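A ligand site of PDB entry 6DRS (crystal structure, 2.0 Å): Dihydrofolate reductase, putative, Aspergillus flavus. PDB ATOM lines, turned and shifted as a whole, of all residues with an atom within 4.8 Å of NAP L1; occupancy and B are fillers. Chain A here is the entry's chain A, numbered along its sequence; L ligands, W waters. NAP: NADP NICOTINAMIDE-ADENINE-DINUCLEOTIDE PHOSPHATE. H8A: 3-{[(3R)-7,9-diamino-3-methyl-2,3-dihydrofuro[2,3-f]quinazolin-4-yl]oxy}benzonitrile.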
ATOM      1  N   ILE A  10      12.185  36.027 -27.942  1.00  0.00           N
ATOM      2  CA  ILE A  10      13.155  36.647 -27.056  1.00  0.00           C
ATOM      3  C   ILE A  10      14.351  35.706 -26.928  1.00  0.00           C
ATOM      4  O   ILE A  10      14.182  34.474 -26.725  1.00  0.00           O
ATOM      5  CB  ILE A  10      12.533  36.978 -25.686  1.00  0.00           C
ATOM      6  CG1 ILE A  10      13.533  37.714 -24.804  1.00  0.00           C
ATOM      7  CG2 ILE A  10      11.945  35.744 -25.018  1.00  0.00           C
ATOM      8  CD1 ILE A  10      12.995  38.102 -23.458  1.00  0.00           C
ATOM      9  N   VAL A  11      15.536  36.301 -27.024  1.00  0.00           N
ATOM     10  CA  VAL A  11      16.787  35.522 -27.192  1.00  0.00           C
ATOM     11  C   VAL A  11      17.952  36.358 -26.669  1.00  0.00           C
ATOM     12  O   VAL A  11      17.898  37.594 -26.718  1.00  0.00           O
ATOM     13  CB  VAL A  11      16.993  35.176 -28.681  1.00  0.00           C
ATOM     14  CG1 VAL A  11      17.335  36.406 -29.509  1.00  0.00           C
ATOM     15  CG2 VAL A  11      18.034  34.075 -28.906  1.00  0.00           C
ATOM     16  N   ALA A  12      18.988  35.683 -26.143  1.00  0.00           N
ATOM     17  CA  ALA A  12      20.293  36.321 -25.934  1.00  0.00           C
ATOM     18  C   ALA A  12      21.278  35.766 -26.995  1.00  0.00           C
ATOM     19  O   ALA A  12      21.303  34.554 -27.243  1.00  0.00           O
ATOM     20  CB  ALA A  12      20.780  36.109 -24.512  1.00  0.00           C
ATOM     21  N   ILE A  26      24.027  31.104 -29.601  1.00  0.00           N
ATOM     22  CA  ILE A  26      22.992  31.108 -28.544  1.00  0.00           C
ATOM     23  C   ILE A  26      23.183  29.925 -27.584  1.00  0.00           C
ATOM     24  O   ILE A  26      22.725  30.016 -26.454  1.00  0.00           O
ATOM     25  CB  ILE A  26      21.573  31.146 -29.139  1.00  0.00           C
ATOM     26  CG1 ILE A  26      21.246  29.862 -29.920  1.00  0.00           C
ATOM     27  CG2 ILE A  26      21.369  32.408 -29.974  1.00  0.00           C
ATOM     28  CD1 ILE A  26      19.783  29.627 -30.131  1.00  0.00           C
ATOM     29  N   GLY A  27      23.897  28.863 -27.992  1.00  0.00           N
ATOM     30  CA  GLY A  27      23.958  27.656 -27.167  1.00  0.00           C
ATOM     31  C   GLY A  27      25.207  26.814 -27.402  1.00  0.00           C
ATOM     32  O   GLY A  27      25.804  26.852 -28.494  1.00  0.00           O
ATOM     33  N   LEU A  28      25.593  26.045 -26.393  1.00  0.00           N
ATOM     34  CA  LEU A  28      26.723  25.097 -26.475  1.00  0.00           C
ATOM     35  C   LEU A  28      26.388  23.911 -25.558  1.00  0.00           C
ATOM     36  O   LEU A  28      26.137  24.121 -24.369  1.00  0.00           O
ATOM     37  CB  LEU A  28      27.999  25.792 -25.961  1.00  0.00           C
ATOM     38  CG  LEU A  28      29.222  24.869 -25.781  1.00  0.00           C
ATOM     39  CD1 LEU A  28      29.799  24.414 -27.118  1.00  0.00           C
ATOM     40  CD2 LEU A  28      30.293  25.531 -24.906  1.00  0.00           C
ATOM     41  N   GLY A  30      23.919  21.873 -25.127  1.00  0.00           N
ATOM     42  CA  GLY A  30      22.570  21.842 -24.529  1.00  0.00           C
ATOM     43  C   GLY A  30      22.356  22.886 -23.425  1.00  0.00           C
ATOM     44  O   GLY A  30      21.331  22.833 -22.757  1.00  0.00           O
ATOM     45  N   THR A  31      23.276  23.803 -23.198  1.00  0.00           N
ATOM     46  CA  THR A  31      23.090  24.897 -22.246  1.00  0.00           C
ATOM     47  C   THR A  31      23.403  26.238 -22.943  1.00  0.00           C
ATOM     48  O   THR A  31      23.551  26.287 -24.189  1.00  0.00           O
ATOM     49  CB  THR A  31      23.959  24.705 -20.991  1.00  0.00           C
ATOM     50  OG1 THR A  31      25.333  24.893 -21.343  1.00  0.00           O
ATOM     51  CG2 THR A  31      23.783  23.370 -20.318  1.00  0.00           C
ATOM     52  N   LEU A  32      23.532  27.312 -22.164  1.00  0.00           N
ATOM     53  CA  LEU A  32      23.945  28.610 -22.746  1.00  0.00           C
ATOM     54  C   LEU A  32      25.463  28.617 -22.938  1.00  0.00           C
ATOM     55  O   LEU A  32      26.163  27.830 -22.325  1.00  0.00           O
ATOM     56  CB  LEU A  32      23.523  29.783 -21.846  1.00  0.00           C
ATOM     57  CG  LEU A  32      22.021  29.918 -21.589  1.00  0.00           C
ATOM     58  CD1 LEU A  32      21.735  31.079 -20.652  1.00  0.00           C
ATOM     59  CD2 LEU A  32      21.245  30.071 -22.901  1.00  0.00           C
ATOM     60  N   TRP A  34      27.632  30.930 -22.039  1.00  0.00           N
ATOM     61  CA  TRP A  34      28.409  31.805 -21.151  1.00  0.00           C
ATOM     62  C   TRP A  34      28.090  31.500 -19.698  1.00  0.00           C
ATOM     63  O   TRP A  34      27.026  30.993 -19.392  1.00  0.00           O
ATOM     64  CB  TRP A  34      28.097  33.291 -21.407  1.00  0.00           C
ATOM     65  CG  TRP A  34      26.630  33.534 -21.606  1.00  0.00           C
ATOM     66  CD1 TRP A  34      25.656  33.586 -20.645  1.00  0.00           C
ATOM     67  CD2 TRP A  34      25.947  33.674 -22.866  1.00  0.00           C
ATOM     68  NE1 TRP A  34      24.431  33.763 -21.215  1.00  0.00           N
ATOM     69  CE2 TRP A  34      24.577  33.828 -22.584  1.00  0.00           C
ATOM     70  CE3 TRP A  34      26.367  33.693 -24.199  1.00  0.00           C
ATOM     71  CZ2 TRP A  34      23.636  34.021 -23.595  1.00  0.00           C
ATOM     72  CZ3 TRP A  34      25.436  33.884 -25.209  1.00  0.00           C
ATOM     73  CH2 TRP A  34      24.080  34.027 -24.894  1.00  0.00           C
ATOM     74  N   GLY A  63      11.152  24.745 -27.583  1.00  0.00           N
ATOM     75  CA  GLY A  63      11.464  23.385 -28.030  1.00  0.00           C
ATOM     76  C   GLY A  63      11.796  22.491 -26.839  1.00  0.00           C
ATOM     77  O   GLY A  63      12.167  22.977 -25.764  1.00  0.00           O
ATOM     78  N   ARG A  64      11.663  21.177 -27.029  1.00  0.00           N
ATOM     79  CA  ARG A  64      11.865  20.240 -25.921  1.00  0.00           C
ATOM     80  C   ARG A  64      13.293  20.363 -25.345  1.00  0.00           C
ATOM     81  O   ARG A  64      13.490  20.214 -24.132  1.00  0.00           O
ATOM     82  CB  ARG A  64      11.404  18.833 -26.297  1.00  0.00           C
ATOM     83  CG  ARG A  64      11.437  17.836 -25.145  1.00  0.00           C
ATOM     84  CD  ARG A  64      12.819  17.254 -24.885  1.00  0.00           C
ATOM     85  NE  ARG A  64      13.304  16.726 -26.158  1.00  0.00           N
ATOM     86  CZ  ARG A  64      14.534  16.313 -26.401  1.00  0.00           C
ATOM     87  NH1 ARG A  64      15.459  16.394 -25.469  1.00  0.00           N
ATOM     88  NH2 ARG A  64      14.825  15.842 -27.600  1.00  0.00           N
ATOM     89  N   LYS A  65      14.291  20.668 -26.192  1.00  0.00           N
ATOM     90  CA  LYS A  65      15.668  20.725 -25.699  1.00  0.00           C
ATOM     91  C   LYS A  65      15.857  21.945 -24.800  1.00  0.00           C
ATOM     92  O   LYS A  65      16.563  21.884 -23.774  1.00  0.00           O
ATOM     93  CB  LYS A  65      16.663  20.702 -26.870  1.00  0.00           C
ATOM     94  CG  LYS A  65      16.960  19.311 -27.399  1.00  0.00           C
ATOM     95  CD  LYS A  65      17.563  19.348 -28.781  1.00  0.00           C
ATOM     96  CE  LYS A  65      18.192  18.045 -29.235  1.00  0.00           C
ATOM     97  NZ  LYS A  65      18.121  17.950 -30.711  1.00  0.00           N
ATOM     98  N   THR A  66      15.207  23.048 -25.154  1.00  0.00           N
ATOM     99  CA  THR A  66      15.258  24.249 -24.321  1.00  0.00           C
ATOM    100  C   THR A  66      14.542  23.976 -22.998  1.00  0.00           C
ATOM    101  O   THR A  66      15.034  24.329 -21.921  1.00  0.00           O
ATOM    102  CB  THR A  66      14.675  25.469 -25.037  1.00  0.00           C
ATOM    103  OG1 THR A  66      15.479  25.723 -26.197  1.00  0.00           O
ATOM    104  CG2 THR A  66      14.662  26.693 -24.152  1.00  0.00           C
ATOM    105  N   SER A  69      16.993  22.191 -21.007  1.00  0.00           N
ATOM    106  CA  SER A  69      18.138  23.035 -20.638  1.00  0.00           C
ATOM    107  C   SER A  69      17.917  23.733 -19.293  1.00  0.00           C
ATOM    108  O   SER A  69      18.899  24.108 -18.653  1.00  0.00           O
ATOM    109  CB  SER A  69      18.452  24.047 -21.689  1.00  0.00           C
ATOM    110  OG  SER A  69      17.514  25.090 -21.710  1.00  0.00           O
ATOM    111  N   VAL A  85       7.271  22.087 -27.142  1.00  0.00           N
ATOM    112  CA  VAL A  85       7.031  21.558 -28.501  1.00  0.00           C
ATOM    113  C   VAL A  85       7.939  20.356 -28.766  1.00  0.00           C
ATOM    114  O   VAL A  85       9.162  20.447 -28.626  1.00  0.00           O
ATOM    115  CB  VAL A  85       7.188  22.636 -29.595  1.00  0.00           C
ATOM    116  CG1 VAL A  85       7.097  22.049 -30.994  1.00  0.00           C
ATOM    117  CG2 VAL A  85       6.164  23.742 -29.419  1.00  0.00           C
ATOM    118  N   THR A  86       7.313  19.240 -29.158  1.00  0.00           N
ATOM    119  CA  THR A  86       7.981  17.955 -29.256  1.00  0.00           C
ATOM    120  C   THR A  86       7.335  17.100 -30.341  1.00  0.00           C
ATOM    121  O   THR A  86       6.197  17.349 -30.784  1.00  0.00           O
ATOM    122  CB  THR A  86       8.010  17.210 -27.907  1.00  0.00           C
ATOM    123  OG1 THR A  86       8.815  16.049 -28.116  1.00  0.00           O
ATOM    124  CG2 THR A  86       6.632  16.773 -27.450  1.00  0.00           C
ATOM    125  N   ARG A  87       8.082  16.092 -30.778  1.00  0.00           N
ATOM    126  CA  ARG A  87       7.528  15.105 -31.714  1.00  0.00           C
ATOM    127  C   ARG A  87       7.115  13.835 -30.942  1.00  0.00           C
ATOM    128  O   ARG A  87       6.628  12.900 -31.540  1.00  0.00           O
ATOM    129  CB  ARG A  87       8.537  14.789 -32.816  1.00  0.00           C
ATOM    130  CG  ARG A  87       8.670  15.904 -33.835  1.00  0.00           C
ATOM    131  CD  ARG A  87       9.468  15.518 -35.058  1.00  0.00           C
ATOM    132  NE  ARG A  87       9.579  16.662 -35.950  1.00  0.00           N
ATOM    133  CZ  ARG A  87      10.560  17.563 -35.896  1.00  0.00           C
ATOM    134  NH1 ARG A  87      11.560  17.414 -35.052  1.00  0.00           N
ATOM    135  NH2 ARG A  87      10.501  18.618 -36.692  1.00  0.00           N
ATOM    136  N   ASP A  88       7.330  13.808 -29.634  1.00  0.00           N
ATOM    137  CA  ASP A  88       6.858  12.691 -28.838  1.00  0.00           C
ATOM    138  C   ASP A  88       5.951  13.214 -27.705  1.00  0.00           C
ATOM    139  O   ASP A  88       6.335  13.205 -26.499  1.00  0.00           O
ATOM    140  CB  ASP A  88       8.021  11.809 -28.375  1.00  0.00           C
ATOM    141  CG  ASP A  88       7.585  10.818 -27.299  1.00  0.00           C
ATOM    142  OD1 ASP A  88       6.452  10.329 -27.385  1.00  0.00           O
ATOM    143  OD2 ASP A  88       8.374  10.577 -26.364  1.00  0.00           O
ATOM    144  N   VAL A  92       6.670  12.763 -23.558  1.00  0.00           N
ATOM    145  CA  VAL A  92       7.107  14.032 -22.935  1.00  0.00           C
ATOM    146  C   VAL A  92       5.992  14.564 -22.000  1.00  0.00           C
ATOM    147  O   VAL A  92       6.272  14.986 -20.851  1.00  0.00           O
ATOM    148  CB  VAL A  92       7.529  15.045 -24.034  1.00  0.00           C
ATOM    149  CG1 VAL A  92       7.859  16.421 -23.470  1.00  0.00           C
ATOM    150  CG2 VAL A  92       8.708  14.508 -24.830  1.00  0.00           C
ATOM    151  N   SER A 133       2.437  19.378 -30.393  1.00  0.00           N
ATOM    152  CA  SER A 133       3.066  18.590 -31.452  1.00  0.00           C
ATOM    153  C   SER A 133       3.770  19.516 -32.472  1.00  0.00           C
ATOM    154  O   SER A 133       4.371  19.051 -33.452  1.00  0.00           O
ATOM    155  CB  SER A 133       2.032  17.746 -32.131  1.00  0.00           C
ATOM    156  OG  SER A 133       1.107  18.588 -32.825  1.00  0.00           O
ATOM    157  N   GLY A 134       3.681  20.820 -32.236  1.00  0.00           N
ATOM    158  CA  GLY A 134       4.226  21.788 -33.156  1.00  0.00           C
ATOM    159  C   GLY A 134       4.026  23.202 -32.638  1.00  0.00           C
ATOM    160  O   GLY A 134       3.359  23.417 -31.620  1.00  0.00           O
ATOM    161  N   ILE A 156      10.566  31.343 -26.810  1.00  0.00           N
ATOM    162  CA  ILE A 156      11.800  31.457 -26.014  1.00  0.00           C
ATOM    163  C   ILE A 156      12.920  30.534 -26.532  1.00  0.00           C
ATOM    164  O   ILE A 156      13.957  30.424 -25.847  1.00  0.00           O
ATOM    165  CB  ILE A 156      11.543  31.264 -24.500  1.00  0.00           C
ATOM    166  CG1 ILE A 156      11.202  29.814 -24.122  1.00  0.00           C
ATOM    167  CG2 ILE A 156      10.444  32.241 -24.073  1.00  0.00           C
ATOM    168  CD1 ILE A 156      11.501  29.463 -22.694  1.00  0.00           C
ATOM    169  N   GLY A 157      12.761  29.947 -27.727  1.00  0.00           N
ATOM    170  CA  GLY A 157      13.830  29.084 -28.255  1.00  0.00           C
ATOM    171  C   GLY A 157      13.526  27.584 -28.223  1.00  0.00           C
ATOM    172  O   GLY A 157      12.431  27.147 -27.824  1.00  0.00           O
ATOM    173  N   GLY A 158      14.494  26.781 -28.686  1.00  0.00           N
ATOM    174  CA  GLY A 158      15.778  27.283 -29.198  1.00  0.00           C
ATOM    175  C   GLY A 158      15.778  27.468 -30.702  1.00  0.00           C
ATOM    176  O   GLY A 158      14.790  27.889 -31.299  1.00  0.00           O
ATOM    177  N   ALA A 159      16.913  27.168 -31.336  1.00  0.00           N
ATOM    178  CA  ALA A 159      17.127  27.473 -32.761  1.00  0.00           C
ATOM    179  C   ALA A 159      16.041  26.844 -33.630  1.00  0.00           C
ATOM    180  O   ALA A 159      15.549  27.503 -34.515  1.00  0.00           O
ATOM    181  CB  ALA A 159      18.514  27.046 -33.207  1.00  0.00           C
ATOM    182  N   GLU A 160      15.646  25.591 -33.372  1.00  0.00           N
ATOM    183  CA  GLU A 160      14.640  24.927 -34.270  1.00  0.00           C
ATOM    184  C   GLU A 160      13.278  25.611 -34.159  1.00  0.00           C
ATOM    185  O   GLU A 160      12.635  25.886 -35.160  1.00  0.00           O
ATOM    186  CB  GLU A 160      14.505  23.429 -33.966  1.00  0.00           C
ATOM    187  CG  GLU A 160      15.767  22.623 -34.252  1.00  0.00           C
ATOM    188  CD  GLU A 160      15.629  21.123 -34.009  1.00  0.00           C
ATOM    189  OE1 GLU A 160      16.645  20.466 -33.617  1.00  0.00           O
ATOM    190  OE2 GLU A 160      14.513  20.596 -34.191  1.00  0.00           O
ATOM    191  N   ILE A 161      12.846  25.875 -32.925  1.00  0.00           N
ATOM    192  CA  ILE A 161      11.582  26.588 -32.664  1.00  0.00           C
ATOM    193  C   ILE A 161      11.638  28.008 -33.245  1.00  0.00           C
ATOM    194  O   ILE A 161      10.668  28.434 -33.890  1.00  0.00           O
ATOM    195  CB  ILE A 161      11.218  26.546 -31.161  1.00  0.00           C
ATOM    196  CG1 ILE A 161      10.376  25.323 -30.806  1.00  0.00           C
ATOM    197  CG2 ILE A 161      10.505  27.811 -30.735  1.00  0.00           C
ATOM    198  CD1 ILE A 161      10.757  24.042 -31.523  1.00  0.00           C
ATOM    199  N   TYR A 162      12.756  28.738 -33.054  1.00  0.00           N
ATOM    200  CA  TYR A 162      12.872  30.108 -33.615  1.00  0.00           C
ATOM    201  C   TYR A 162      12.725  30.064 -35.143  1.00  0.00           C
ATOM    202  O   TYR A 162      12.044  30.909 -35.748  1.00  0.00           O
ATOM    203  CB  TYR A 162      14.228  30.739 -33.329  1.00  0.00           C
ATOM    204  CG  TYR A 162      14.507  31.183 -31.910  1.00  0.00           C
ATOM    205  CD1 TYR A 162      13.581  31.898 -31.174  1.00  0.00           C
ATOM    206  CD2 TYR A 162      15.721  30.886 -31.324  1.00  0.00           C
ATOM    207  CE1 TYR A 162      13.852  32.317 -29.885  1.00  0.00           C
ATOM    208  CE2 TYR A 162      16.006  31.273 -30.021  1.00  0.00           C
ATOM    209  CZ  TYR A 162      15.077  32.018 -29.308  1.00  0.00           C
ATOM    210  OH  TYR A 162      15.380  32.370 -28.032  1.00  0.00           O
ATOM    211  N   THR A 164      11.155  27.891 -36.866  1.00  0.00           N
ATOM    212  CA  THR A 164       9.727  27.677 -37.165  1.00  0.00           C
ATOM    213  C   THR A 164       8.930  28.978 -36.994  1.00  0.00           C
ATOM    214  O   THR A 164       8.120  29.326 -37.867  1.00  0.00           O
ATOM    215  CB  THR A 164       9.097  26.569 -36.318  1.00  0.00           C
ATOM    216  OG1 THR A 164       9.943  25.425 -36.432  1.00  0.00           O
ATOM    217  CG2 THR A 164       7.719  26.197 -36.813  1.00  0.00           C
ATOM    218  N   THR A 197      25.085  26.094 -31.349  1.00  0.00           N
ATOM    219  CA  THR A 197      23.708  26.477 -31.748  1.00  0.00           C
ATOM    220  C   THR A 197      23.674  27.986 -31.992  1.00  0.00           C
ATOM    221  O   THR A 197      24.246  28.721 -31.200  1.00  0.00           O
ATOM    222  CB  THR A 197      22.690  26.043 -30.673  1.00  0.00           C
ATOM    223  OG1 THR A 197      23.050  24.729 -30.240  1.00  0.00           O
ATOM    224  CG2 THR A 197      21.259  26.086 -31.169  1.00  0.00           C
HETATM  225  PA  NAP L   1      15.166  23.498 -29.493  1.00  0.00           P
HETATM  226  O1A NAP L   1      15.089  24.102 -28.115  1.00  0.00           O
HETATM  227  O2A NAP L   1      14.747  24.099 -30.778  1.00  0.00           O
HETATM  228  O5B NAP L   1      14.481  22.024 -29.407  1.00  0.00           O
HETATM  229  C5B NAP L   1      14.599  21.021 -30.423  1.00  0.00           C
HETATM  230  C4B NAP L   1      13.528  19.998 -30.097  1.00  0.00           C
HETATM  231  O4B NAP L   1      12.246  20.598 -30.235  1.00  0.00           O
HETATM  232  C3B NAP L   1      13.485  18.812 -31.051  1.00  0.00           C
HETATM  233  O3B NAP L   1      14.417  17.795 -30.638  1.00  0.00           O
HETATM  234  C2B NAP L   1      12.042  18.353 -30.914  1.00  0.00           C
HETATM  235  O2B NAP L   1      11.848  17.735 -29.650  1.00  0.00           O
HETATM  236  C1B NAP L   1      11.290  19.666 -30.758  1.00  0.00           C
HETATM  237  N9A NAP L   1      10.855  20.168 -32.050  1.00  0.00           N
HETATM  238  C8A NAP L   1      11.629  21.013 -32.764  1.00  0.00           C
HETATM  239  N7A NAP L   1      11.002  21.330 -33.916  1.00  0.00           N
HETATM  240  C5A NAP L   1       9.817  20.689 -33.949  1.00  0.00           C
HETATM  241  C6A NAP L   1       8.680  20.613 -34.897  1.00  0.00           C
HETATM  242  N6A NAP L   1       8.761  21.338 -36.020  1.00  0.00           N
HETATM  243  N1A NAP L   1       7.606  19.843 -34.617  1.00  0.00           N
HETATM  244  C2A NAP L   1       7.579  19.161 -33.460  1.00  0.00           C
HETATM  245  N3A NAP L   1       8.589  19.186 -32.544  1.00  0.00           N
HETATM  246  C4A NAP L   1       9.722  19.910 -32.714  1.00  0.00           C
HETATM  247  O3  NAP L   1      16.698  22.927 -29.589  1.00  0.00           O
HETATM  248  PN  NAP L   1      18.021  23.620 -30.239  1.00  0.00           P
HETATM  249  O1N NAP L   1      17.709  24.346 -31.479  1.00  0.00           O
HETATM  250  O2N NAP L   1      19.006  22.477 -30.236  1.00  0.00           O
HETATM  251  O5D NAP L   1      18.446  24.657 -29.100  1.00  0.00           O
HETATM  252  C5D NAP L   1      18.747  24.219 -27.797  1.00  0.00           C
HETATM  253  C4D NAP L   1      19.992  25.013 -27.474  1.00  0.00           C
HETATM  254  O4D NAP L   1      19.705  26.395 -27.670  1.00  0.00           O
HETATM  255  C3D NAP L   1      20.508  24.858 -26.051  1.00  0.00           C
HETATM  256  O3D NAP L   1      21.950  24.933 -26.126  1.00  0.00           O
HETATM  257  C2D NAP L   1      19.939  26.078 -25.374  1.00  0.00           C
HETATM  258  O2D NAP L   1      20.723  26.433 -24.262  1.00  0.00           O
HETATM  259  C1D NAP L   1      19.988  27.124 -26.468  1.00  0.00           C
HETATM  260  N1N NAP L   1      19.016  28.212 -26.245  1.00  0.00           N
HETATM  261  C2N NAP L   1      19.502  29.465 -26.099  1.00  0.00           C
HETATM  262  C3N NAP L   1      18.644  30.565 -25.873  1.00  0.00           C
HETATM  263  C7N NAP L   1      19.237  31.971 -25.723  1.00  0.00           C
HETATM  264  O7N NAP L   1      18.489  32.956 -25.628  1.00  0.00           O
HETATM  265  N7N NAP L   1      20.573  32.099 -25.703  1.00  0.00           N
HETATM  266  C4N NAP L   1      17.270  30.327 -25.750  1.00  0.00           C
HETATM  267  C5N NAP L   1      16.805  29.010 -25.899  1.00  0.00           C
HETATM  268  C6N NAP L   1      17.694  27.966 -26.135  1.00  0.00           C
HETATM  269  P2B NAP L   1      11.886  16.130 -29.480  1.00  0.00           P
HETATM  270  O1X NAP L   1      13.335  15.719 -29.757  1.00  0.00           O
HETATM  271  O2X NAP L   1      11.625  15.947 -28.007  1.00  0.00           O
HETATM  272  O3X NAP L   1      10.912  15.769 -30.553  1.00  0.00           O
HETATM  273  C2  H8A L   2      17.557  31.740 -20.200  1.00  0.00           C
HETATM  274  C3  H8A L   2      17.890  33.086 -20.421  1.00  0.00           C
HETATM  275  C4  H8A L   2      17.380  33.760 -21.540  1.00  0.00           C
HETATM  276  C5  H8A L   2      16.552  33.094 -22.477  1.00  0.00           C
HETATM  277  C6  H8A L   2      16.221  31.740 -22.205  1.00  0.00           C
HETATM  278  C7  H8A L   2      16.741  31.104 -21.117  1.00  0.00           C
HETATM  279  C8  H8A L   2      16.062  33.796 -23.556  1.00  0.00           C
HETATM  280  O1  H8A L   2      18.031  31.071 -19.116  1.00  0.00           O
HETATM  281  C10 H8A L   2      17.181  35.723 -22.850  1.00  0.00           C
HETATM  282  C14 H8A L   2      17.288  30.806 -17.978  1.00  0.00           C
HETATM  283  C15 H8A L   2      17.723  29.779 -17.119  1.00  0.00           C
HETATM  284  C16 H8A L   2      16.982  29.484 -15.959  1.00  0.00           C
HETATM  285  C17 H8A L   2      15.811  30.223 -15.668  1.00  0.00           C
HETATM  286  C18 H8A L   2      15.355  31.254 -16.510  1.00  0.00           C
HETATM  287  N9  H8A L   2      16.393  35.093 -23.734  1.00  0.00           N
HETATM  288  N11 H8A L   2      17.691  35.067 -21.792  1.00  0.00           N
HETATM  289  N12 H8A L   2      15.163  33.132 -24.491  1.00  0.00           N
HETATM  290  N13 H8A L   2      17.557  37.125 -23.009  1.00  0.00           N
HETATM  291  C19 H8A L   2      16.101  31.528 -17.667  1.00  0.00           C
HETATM  292  C20 H8A L   2      14.235  31.934 -16.219  1.00  0.00           C
HETATM  293  N21 H8A L   2      13.203  32.496 -15.971  1.00  0.00           N
HETATM  294  C22 H8A L   2      16.297  29.710 -21.058  1.00  0.00           C
HETATM  295  C23 H8A L   2      15.612  29.571 -22.423  1.00  0.00           C
HETATM  296  O24 H8A L   2      15.431  30.902 -22.946  1.00  0.00           O
HETATM  297  C25 H8A L   2      15.153  29.619 -20.069  1.00  0.00           C
HETATM  298  O   HOH W   1      21.002  21.788 -27.900  1.00  0.00           O
HETATM  299  O   HOH W   2      19.020  27.455 -22.417  1.00  0.00           O
HETATM  300  O   HOH W   3      16.201  18.013 -32.860  1.00  0.00           O
HETATM  301  O   HOH W   4      19.610  23.668 -33.543  1.00  0.00           O
HETATM  302  O   HOH W   5      11.619  21.093 -36.785  1.00  0.00           O
HETATM  303  O   HOH W   6      23.529  23.022 -27.601  1.00  0.00           O
HETATM  304  O   HOH W   7      18.595  20.611 -31.991  1.00  0.00           O
HETATM  305  O   HOH W   8      12.253  15.353 -33.012  1.00  0.00           O
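Water W7 lies within hydrogen-bond range of the side-chain carboxylate (OE1) of Glu 160, an oxygen (O2N) of NAP L1 and the side-chain amino group (NZ) of Lys 65. Water W2 lies within hydrogen-bond range of O2D of NAP L1 (2.7 Å) and OG of Ser 69 (2.9 Å). Water W8 lies within hydrogen-bond range of O3X of NAP L1 (2.8 Å) and NH1 of Arg 87 (3.0 Å). Water W3 lies within hydrogen-bond range of the side-chain carboxylate of Glu 160 (2.6 Å), an oxygen (O3B) of NAP L1 (2.9 Å) and the side-chain amino group of Lys 65 (2.9 Å). Water W6 lies within hydrogen-bond range of N of Gly 30, O3D of NAP L1 and OG1 of Thr 197. Water W5 lies within hydrogen-bond range of NH2 of Arg 87 and N7A of NAP L1.
The side-chain hydroxyl (OG1) of Thr 86 is in hydrogen-bond range of the backbone NH (N) of Asp 88, 3.1 Å away. The backbone NH (N) of Gly 158 is in hydrogen-bond range of the side-chain hydroxyl (OG1) of Thr 66 (2.9 Å). OG1 of Thr 31 lies within hydrogen-bond range of O of Leu 28. The backbone NH of Gly 63 is in hydrogen-bond range of the backbone carbonyl oxygen of Gly 157 (2.7 Å). OG of Ser 69 sits at hydrogen-bond distance from O of Thr 66. The backbone NH of Ile 26 sits at hydrogen-bond distance from the backbone carbonyl oxygen of Thr 197, 2.9 Å away. O of Gly 27 sits at hydrogen-bond distance from N of Thr 197 (3.0 Å). The backbone carbonyl oxygen (O) of Ile 10 lies within hydrogen-bond range of the side-chain hydroxyl (OH) of Tyr 162 (2.8 Å).
O of Val 85 lies close to O4B of NAP L1. Residues that only touch NAP L1: Val 11, Gly 27, Leu 28, Gly 30, Leu 32, Gly 63, Ser 133, Ile 156, Gly 157, Tyr 162 and Thr 197. Hydrophobic or aromatic side chains within 4 Å of NAP L1: Val 11, Ile 26, Leu 32, Val 85, Ala 159 and Ile 161.
The backbone NH (N) of Ile 161 is in hydrogen-bond range of an oxygen (O2A) of NAP L1, 3.4 Å away. The backbone carbonyl oxygen (O) of Ile 156 lies within hydrogen-bond range of a nitrogen (N12) of H8A L2 (3.3 Å). The backbone NH (N) of Thr 31 sits at hydrogen-bond distance from an oxygen (O3D) of NAP L1, 3.4 Å away. O1N of NAP L1 sits at hydrogen-bond distance from N of Ala 159. N of Lys 65 is in hydrogen-bond range of O5B of NAP L1 (3.5 Å). N of Thr 66 is in hydrogen-bond range of O1A of NAP L1 (3.1 Å). O of Ala 12 sits at hydrogen-bond distance from N7N of NAP L1 (3.0 Å). N of Ala 12 is in hydrogen-bond range of O7N of NAP L1 (2.8 Å). An oxygen (O1A) of NAP L1 lies within hydrogen-bond range of the side-chain hydroxyl (OG1) of Thr 66 (2.5 Å). The backbone NH of Arg 64 lies within hydrogen-bond range of an oxygen (O4B) of NAP L1, 3.3 Å away. The backbone carbonyl oxygen (O) of Thr 31 is in hydrogen-bond range of an oxygen (O2D) of NAP L1, at 2.8 Å. The backbone carbonyl oxygen (O) of Ile 26 lies within hydrogen-bond range of a nitrogen (N7N) of NAP L1 (3.1 Å). N of Arg 87 lies within hydrogen-bond range of O3X of NAP L1, 2.9 Å away. N12 of H8A L2 sits at hydrogen-bond distance from O of Ile 10 (2.8 Å). N of Glu 160 lies within hydrogen-bond range of O1N of NAP L1. An oxygen (O2X) of NAP L1 is in salt-bridge range of the guanidinium group of Arg 64 (2.6 Å). An oxygen (O2X) of NAP L1 is in hydrogen-bond range of the side-chain hydroxyl (OG1) of Thr 86 (2.8 Å). An oxygen (O1A) of NAP L1 sits at hydrogen-bond distance from the backbone NH of Gly 158 (2.8 Å).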
